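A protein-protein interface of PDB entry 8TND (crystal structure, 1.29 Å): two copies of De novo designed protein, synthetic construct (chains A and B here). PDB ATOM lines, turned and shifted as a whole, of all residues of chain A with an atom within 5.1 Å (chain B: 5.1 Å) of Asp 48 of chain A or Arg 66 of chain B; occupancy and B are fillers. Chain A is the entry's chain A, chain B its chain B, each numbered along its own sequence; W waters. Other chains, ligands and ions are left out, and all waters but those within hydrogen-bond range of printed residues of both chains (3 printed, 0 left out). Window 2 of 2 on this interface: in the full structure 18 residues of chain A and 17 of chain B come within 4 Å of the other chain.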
ATOM      1  N   LEU A  43      -3.111  17.747 -11.529  1.00  0.00           N
ATOM      2  CA  LEU A  43      -4.036  16.956 -12.316  1.00  0.00           C
ATOM      3  C   LEU A  43      -5.421  17.578 -12.290  1.00  0.00           C
ATOM      4  O   LEU A  43      -6.095  17.647 -13.336  1.00  0.00           O
ATOM      5  CB  LEU A  43      -4.034  15.510 -11.826  1.00  0.00           C
ATOM      6  CG  LEU A  43      -5.043  14.590 -12.473  1.00  0.00           C
ATOM      7  CD1 LEU A  43      -4.793  14.483 -13.954  1.00  0.00           C
ATOM      8  CD2 LEU A  43      -5.014  13.198 -11.776  1.00  0.00           C
ATOM      9  N   ALA A  44      -5.884  18.011 -11.126  1.00  0.00           N
ATOM     10  CA  ALA A  44      -7.225  18.592 -11.037  1.00  0.00           C
ATOM     11  C   ALA A  44      -7.344  19.806 -11.933  1.00  0.00           C
ATOM     12  O   ALA A  44      -8.368  19.993 -12.609  1.00  0.00           O
ATOM     13  CB  ALA A  44      -7.551  18.977  -9.594  1.00  0.00           C
ATOM     14  N   THR A  45      -6.321  20.646 -11.965  1.00  0.00           N
ATOM     15  CA  THR A  45      -6.356  21.843 -12.807  1.00  0.00           C
ATOM     16  C   THR A  45      -6.419  21.453 -14.270  1.00  0.00           C
ATOM     17  O   THR A  45      -7.188  22.034 -15.055  1.00  0.00           O
ATOM     18  CB  THR A  45      -5.136  22.717 -12.498  1.00  0.00           C
ATOM     19  OG1 THR A  45      -5.267  23.203 -11.152  1.00  0.00           O
ATOM     20  CG2 THR A  45      -5.007  23.901 -13.423  1.00  0.00           C
ATOM     21  N   TYR A  46      -5.598  20.503 -14.672  1.00  0.00           N
ATOM     22  CA  TYR A  46      -5.577  20.131 -16.069  1.00  0.00           C
ATOM     23  C   TYR A  46      -6.850  19.416 -16.480  1.00  0.00           C
ATOM     24  O   TYR A  46      -7.330  19.618 -17.605  1.00  0.00           O
ATOM     25  CB  TYR A  46      -4.362  19.268 -16.374  1.00  0.00           C
ATOM     26  CG  TYR A  46      -3.068  20.060 -16.318  1.00  0.00           C
ATOM     27  CD1 TYR A  46      -2.949  21.281 -16.976  1.00  0.00           C
ATOM     28  CD2 TYR A  46      -1.974  19.599 -15.598  1.00  0.00           C
ATOM     29  CE1 TYR A  46      -1.774  22.015 -16.933  1.00  0.00           C
ATOM     30  CE2 TYR A  46      -0.786  20.347 -15.529  1.00  0.00           C
ATOM     31  CZ  TYR A  46      -0.704  21.537 -16.213  1.00  0.00           C
ATOM     32  OH  TYR A  46       0.500  22.238 -16.184  1.00  0.00           O
ATOM     33  N   LEU A  47      -7.445  18.627 -15.592  1.00  0.00           N
ATOM     34  CA  LEU A  47      -8.720  17.996 -15.908  1.00  0.00           C
ATOM     35  C   LEU A  47      -9.826  19.032 -16.034  1.00  0.00           C
ATOM     36  O   LEU A  47     -10.698  18.910 -16.913  1.00  0.00           O
ATOM     37  CB  LEU A  47      -9.071  16.962 -14.845  1.00  0.00           C
ATOM     38  CG  LEU A  47      -8.219  15.703 -14.883  1.00  0.00           C
ATOM     39  CD1 LEU A  47      -8.596  14.818 -13.703  1.00  0.00           C
ATOM     40  CD2 LEU A  47      -8.359  14.948 -16.162  1.00  0.00           C
ATOM     41  N   ASP A  48      -9.801  20.066 -15.222  1.00  0.00           N
ATOM     42  CA  ASP A  48     -10.835  21.086 -15.360  1.00  0.00           C
ATOM     43  C   ASP A  48     -10.672  21.836 -16.665  1.00  0.00           C
ATOM     44  O   ASP A  48     -11.659  22.155 -17.346  1.00  0.00           O
ATOM     45  CB  ASP A  48     -10.764  22.053 -14.199  1.00  0.00           C
ATOM     46  CG  ASP A  48     -11.301  21.466 -12.925  1.00  0.00           C
ATOM     47  OD1 ASP A  48     -11.987  20.417 -12.962  1.00  0.00           O
ATOM     48  OD2 ASP A  48     -11.080  22.121 -11.909  1.00  0.00           O
ATOM     49  N   GLN A  49      -9.450  22.124 -17.057  1.00  0.00           N
ATOM     50  CA  GLN A  49      -9.220  22.737 -18.359  1.00  0.00           C
ATOM     51  C   GLN A  49      -9.688  21.821 -19.479  1.00  0.00           C
ATOM     52  O   GLN A  49     -10.362  22.258 -20.424  1.00  0.00           O
ATOM     53  CB  GLN A  49      -7.753  23.083 -18.535  1.00  0.00           C
ATOM     54  CG  GLN A  49      -7.301  24.243 -17.698  1.00  0.00           C
ATOM     55  CD  GLN A  49      -7.919  25.570 -18.129  1.00  0.00           C
ATOM     56  OE1 GLN A  49      -7.850  25.950 -19.293  1.00  0.00           O
ATOM     57  NE2 GLN A  49      -8.497  26.288 -17.182  1.00  0.00           N
ATOM     58  N   ALA A  50      -9.335  20.548 -19.424  1.00  0.00           N
ATOM     59  CA  ALA A  50      -9.781  19.606 -20.442  1.00  0.00           C
ATOM     60  C   ALA A  50     -11.298  19.566 -20.531  1.00  0.00           C
ATOM     61  O   ALA A  50     -11.872  19.576 -21.631  1.00  0.00           O
ATOM     62  CB  ALA A  50      -9.232  18.213 -20.143  1.00  0.00           C
ATOM     63  N   ALA A  51     -11.982  19.557 -19.396  1.00  0.00           N
ATOM     64  CA  ALA A  51     -13.444  19.516 -19.417  1.00  0.00           C
ATOM     65  C   ALA A  51     -14.017  20.767 -20.072  1.00  0.00           C
ATOM     66  O   ALA A  51     -15.023  20.695 -20.801  1.00  0.00           O
ATOM     67  CB  ALA A  51     -13.989  19.366 -17.999  1.00  0.00           C
ATOM     68  N   SER A  52     -13.413  21.916 -19.819  1.00  0.00           N
ATOM     69  CA  SER A  52     -13.896  23.149 -20.432  1.00  0.00           C
ATOM     70  C   SER A  52     -13.724  23.085 -21.940  1.00  0.00           C
ATOM     71  O   SER A  52     -14.653  23.404 -22.699  1.00  0.00           O
ATOM     72  CB  SER A  52     -13.159  24.327 -19.822  1.00  0.00           C
ATOM     73  OG  SER A  52     -13.535  25.545 -20.448  1.00  0.00           O
ATOM     74  N   VAL A 105     -13.037  12.662 -14.587  1.00  0.00           N
ATOM     75  CA  VAL A 105     -12.952  13.795 -13.673  1.00  0.00           C
ATOM     76  C   VAL A 105     -13.579  13.456 -12.327  1.00  0.00           C
ATOM     77  O   VAL A 105     -13.019  13.774 -11.262  1.00  0.00           O
ATOM     78  CB  VAL A 105     -13.589  15.048 -14.303  1.00  0.00           C
ATOM     79  CG1 VAL A 105     -13.623  16.204 -13.318  1.00  0.00           C
ATOM     80  CG2 VAL A 105     -12.826  15.438 -15.551  1.00  0.00           C
ATOM     81  N   ALA A 109     -11.718  13.171  -8.644  1.00  0.00           N
ATOM     82  CA  ALA A 109     -12.203  13.937  -7.502  1.00  0.00           C
ATOM     83  C   ALA A 109     -12.542  13.014  -6.331  1.00  0.00           C
ATOM     84  O   ALA A 109     -12.308  13.377  -5.175  1.00  0.00           O
ATOM     85  CB  ALA A 109     -13.441  14.751  -7.897  1.00  0.00           C
ATOM     86  N   GLN B  59     -19.040  21.524 -13.131  1.00  0.00           N
ATOM     87  CA  GLN B  59     -17.760  21.986 -12.594  1.00  0.00           C
ATOM     88  C   GLN B  59     -17.877  22.298 -11.120  1.00  0.00           C
ATOM     89  O   GLN B  59     -16.989  21.945 -10.326  1.00  0.00           O
ATOM     90  CB  GLN B  59     -17.333  23.229 -13.370  1.00  0.00           C
ATOM     91  CG  GLN B  59     -15.983  23.804 -12.971  1.00  0.00           C
ATOM     92  CD  GLN B  59     -14.854  22.814 -12.965  1.00  0.00           C
ATOM     93  OE1 GLN B  59     -14.751  21.934 -13.823  1.00  0.00           O
ATOM     94  NE2 GLN B  59     -13.974  22.954 -11.961  1.00  0.00           N
ATOM     95  N   VAL B  62     -17.976  19.053  -9.157  1.00  0.00           N
ATOM     96  CA  VAL B  62     -16.625  18.503  -9.018  1.00  0.00           C
ATOM     97  C   VAL B  62     -15.861  19.251  -7.936  1.00  0.00           C
ATOM     98  O   VAL B  62     -15.212  18.636  -7.072  1.00  0.00           O
ATOM     99  CB  VAL B  62     -15.896  18.595 -10.373  1.00  0.00           C
ATOM    100  CG1 VAL B  62     -14.401  18.335 -10.184  1.00  0.00           C
ATOM    101  CG2 VAL B  62     -16.483  17.625 -11.391  1.00  0.00           C
ATOM    102  N   GLU B  63     -15.918  20.578  -7.936  1.00  0.00           N
ATOM    103  CA  GLU B  63     -15.211  21.353  -6.924  1.00  0.00           C
ATOM    104  C   GLU B  63     -15.725  21.029  -5.529  1.00  0.00           C
ATOM    105  O   GLU B  63     -14.951  21.034  -4.563  1.00  0.00           O
ATOM    106  CB  GLU B  63     -15.340  22.851  -7.181  1.00  0.00           C
ATOM    107  CG  GLU B  63     -14.802  23.323  -8.476  1.00  0.00           C
ATOM    108  CD  GLU B  63     -15.040  24.809  -8.724  1.00  0.00           C
ATOM    109  OE1 GLU B  63     -15.344  25.558  -7.752  1.00  0.00           O
ATOM    110  OE2 GLU B  63     -14.881  25.235  -9.892  1.00  0.00           O
ATOM    111  N   THR B  64     -17.027  20.794  -5.387  1.00  0.00           N
ATOM    112  CA  THR B  64     -17.631  20.463  -4.102  1.00  0.00           C
ATOM    113  C   THR B  64     -17.083  19.141  -3.585  1.00  0.00           C
ATOM    114  O   THR B  64     -16.710  19.032  -2.396  1.00  0.00           O
ATOM    115  CB  THR B  64     -19.148  20.427  -4.314  1.00  0.00           C
ATOM    116  OG1 THR B  64     -19.616  21.739  -4.601  1.00  0.00           O
ATOM    117  CG2 THR B  64     -19.860  19.955  -3.073  1.00  0.00           C
ATOM    118  N   VAL B  65     -17.018  18.121  -4.438  1.00  0.00           N
ATOM    119  CA  VAL B  65     -16.415  16.850  -4.050  1.00  0.00           C
ATOM    120  C   VAL B  65     -14.963  17.060  -3.643  1.00  0.00           C
ATOM    121  O   VAL B  65     -14.512  16.549  -2.610  1.00  0.00           O
ATOM    122  CB  VAL B  65     -16.572  15.787  -5.154  1.00  0.00           C
ATOM    123  CG1 VAL B  65     -15.677  14.553  -4.888  1.00  0.00           C
ATOM    124  CG2 VAL B  65     -18.035  15.383  -5.277  1.00  0.00           C
ATOM    125  N   ARG B  66     -14.203  17.830  -4.422  1.00  0.00           N
ATOM    126  CA  ARG B  66     -12.788  17.994  -4.109  1.00  0.00           C
ATOM    127  C   ARG B  66     -12.622  18.675  -2.766  1.00  0.00           C
ATOM    128  O   ARG B  66     -11.739  18.302  -1.972  1.00  0.00           O
ATOM    129  CB  ARG B  66     -12.104  18.811  -5.201  1.00  0.00           C
ATOM    130  CG  ARG B  66     -11.846  18.037  -6.467  1.00  0.00           C
ATOM    131  CD  ARG B  66     -11.036  18.896  -7.383  1.00  0.00           C
ATOM    132  NE  ARG B  66     -11.061  18.413  -8.760  1.00  0.00           N
ATOM    133  CZ  ARG B  66     -11.076  19.194  -9.830  1.00  0.00           C
ATOM    134  NH1 ARG B  66     -11.147  20.507  -9.719  1.00  0.00           N
ATOM    135  NH2 ARG B  66     -10.983  18.638 -11.039  1.00  0.00           N
ATOM    136  N   LEU B  67     -13.446  19.676  -2.472  1.00  0.00           N
ATOM    137  CA  LEU B  67     -13.356  20.365  -1.189  1.00  0.00           C
ATOM    138  C   LEU B  67     -13.729  19.446  -0.031  1.00  0.00           C
ATOM    139  O   LEU B  67     -13.095  19.502   1.043  1.00  0.00           O
ATOM    140  CB  LEU B  67     -14.238  21.609  -1.175  1.00  0.00           C
ATOM    141  CG  LEU B  67     -13.670  22.803  -1.929  1.00  0.00           C
ATOM    142  CD1 LEU B  67     -14.735  23.823  -2.285  1.00  0.00           C
ATOM    143  CD2 LEU B  67     -12.547  23.486  -1.147  1.00  0.00           C
ATOM    144  N   LEU B  68     -14.752  18.622  -0.189  1.00  0.00           N
ATOM    145  CA  LEU B  68     -15.133  17.718   0.894  1.00  0.00           C
ATOM    146  C   LEU B  68     -14.122  16.595   1.056  1.00  0.00           C
ATOM    147  O   LEU B  68     -13.917  16.116   2.182  1.00  0.00           O
ATOM    148  CB  LEU B  68     -16.539  17.188   0.649  1.00  0.00           C
ATOM    149  CG  LEU B  68     -17.582  18.202   1.068  1.00  0.00           C
ATOM    150  CD1 LEU B  68     -18.918  17.928   0.431  1.00  0.00           C
ATOM    151  CD2 LEU B  68     -17.744  18.240   2.581  1.00  0.00           C
ATOM    152  N   ALA B  69     -13.475  16.157  -0.017  1.00  0.00           N
ATOM    153  CA  ALA B  69     -12.375  15.215   0.119  1.00  0.00           C
ATOM    154  C   ALA B  69     -11.240  15.847   0.898  1.00  0.00           C
ATOM    155  O   ALA B  69     -10.612  15.184   1.740  1.00  0.00           O
ATOM    156  CB  ALA B  69     -11.890  14.775  -1.261  1.00  0.00           C
ATOM    157  N   GLU B  70     -10.976  17.131   0.673  1.00  0.00           N
ATOM    158  CA  GLU B  70      -9.939  17.813   1.433  1.00  0.00           C
ATOM    159  C   GLU B  70     -10.349  17.937   2.896  1.00  0.00           C
ATOM    160  O   GLU B  70      -9.536  17.684   3.801  1.00  0.00           O
ATOM    161  CB  GLU B  70      -9.657  19.181   0.813  1.00  0.00           C
ATOM    162  CG  GLU B  70      -8.737  20.090   1.618  1.00  0.00           C
ATOM    163  CD  GLU B  70      -8.433  21.404   0.907  1.00  0.00           C
ATOM    164  OE1 GLU B  70      -7.284  21.892   1.032  1.00  0.00           O
ATOM    165  OE2 GLU B  70      -9.322  21.932   0.199  1.00  0.00           O
HETATM  166  O   HOH W   1     -11.188  15.884 -10.670  1.00  0.00           O
HETATM  167  O   HOH W   2     -14.071  23.006 -16.252  1.00  0.00           O
HETATM  168  O   HOH W   3     -14.392  19.554 -14.146  1.00  0.00           O
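The guanidinium group (NH1) of Arg 66 of chain B is in salt-bridge range of the side-chain carboxylate (OD2) of Asp 48 of chain A, 2.7 Å away.
The backbone carbonyl oxygen (O) of Ala 44 of chain A lies within hydrogen-bond range of the guanidinium group (NH2) of Arg 66 of chain B (3.3 Å).
OD2 of Asp 48 of chain A sits at hydrogen-bond distance from NE2 of Gln 59 of chain B.
The side-chain amide nitrogen (NE2) of Gln 59 of chain B sits at hydrogen-bond distance from the side-chain carboxylate (OE2) of Glu 63 of chain B, at 3.2 Å.
Among the printed residues, pairs that only touch across the chains: Val 105 of chain A with Val 62 of chain B, Ala 109 of chain A with Val 65 of chain B and Ala 109 of chain A with Arg 66 of chain B.
Asp 48 of chain A touches two residues of chain B.
Of chain A, only Ala 44 (3.3 Å), Asp 48 (2.7 Å) and Ala 109 (3.9 Å) come within 4 Å of Arg 66 of chain B.
Printed residues of chain B within 4 Å of Ala 109 of chain A: Val 65 and Arg 66.
Of the printed residues of chain A, Val 65 of chain B touches Ala 109 (3.6 Å).
Leu 47 of chain A touches none of the printed residues of chain B.
Of the 10 printed residues of chain B, 4 touch a printed residue of chain A.
Hydrophobic or aromatic side chains of chain B that line the printed part of chain A: Val 62 and Val 65.
Of the 12 printed residues of chain A, 4 touch a printed residue of chain B.
Printed residues of chain A that touch a printed residue of chain B: Ala 44, Asp 48, Val 105 and Ala 109.
Hydrophobic or aromatic side chains of chain A that line the printed part of chain B: Ala 44, Val 105 and Ala 109.
No position is printed for both chains.
Of the 6 pairs that touch across the chains among the printed residues, none has its exchanged pair printed and touching as well.
Water W3 lies within hydrogen-bond range of OE1 of Gln 59 of chain B (2.4 Å) and OD1 of Asp 48 of chain A (2.8 Å).
Water W2 bridges the side-chain amide oxygen of Gln 59 of chain B (2.7 Å) and the backbone carbonyl oxygen of Asp 48 of chain A (2.8 Å).
Water W1 lies within hydrogen-bond range of the guanidinium group (NH2) of Arg 66 of chain B (2.8 Å), the backbone carbonyl oxygen (O) of Val 105 of chain A (2.9 Å) and the backbone NH (N) of Ala 109 of chain A (3.4 Å).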
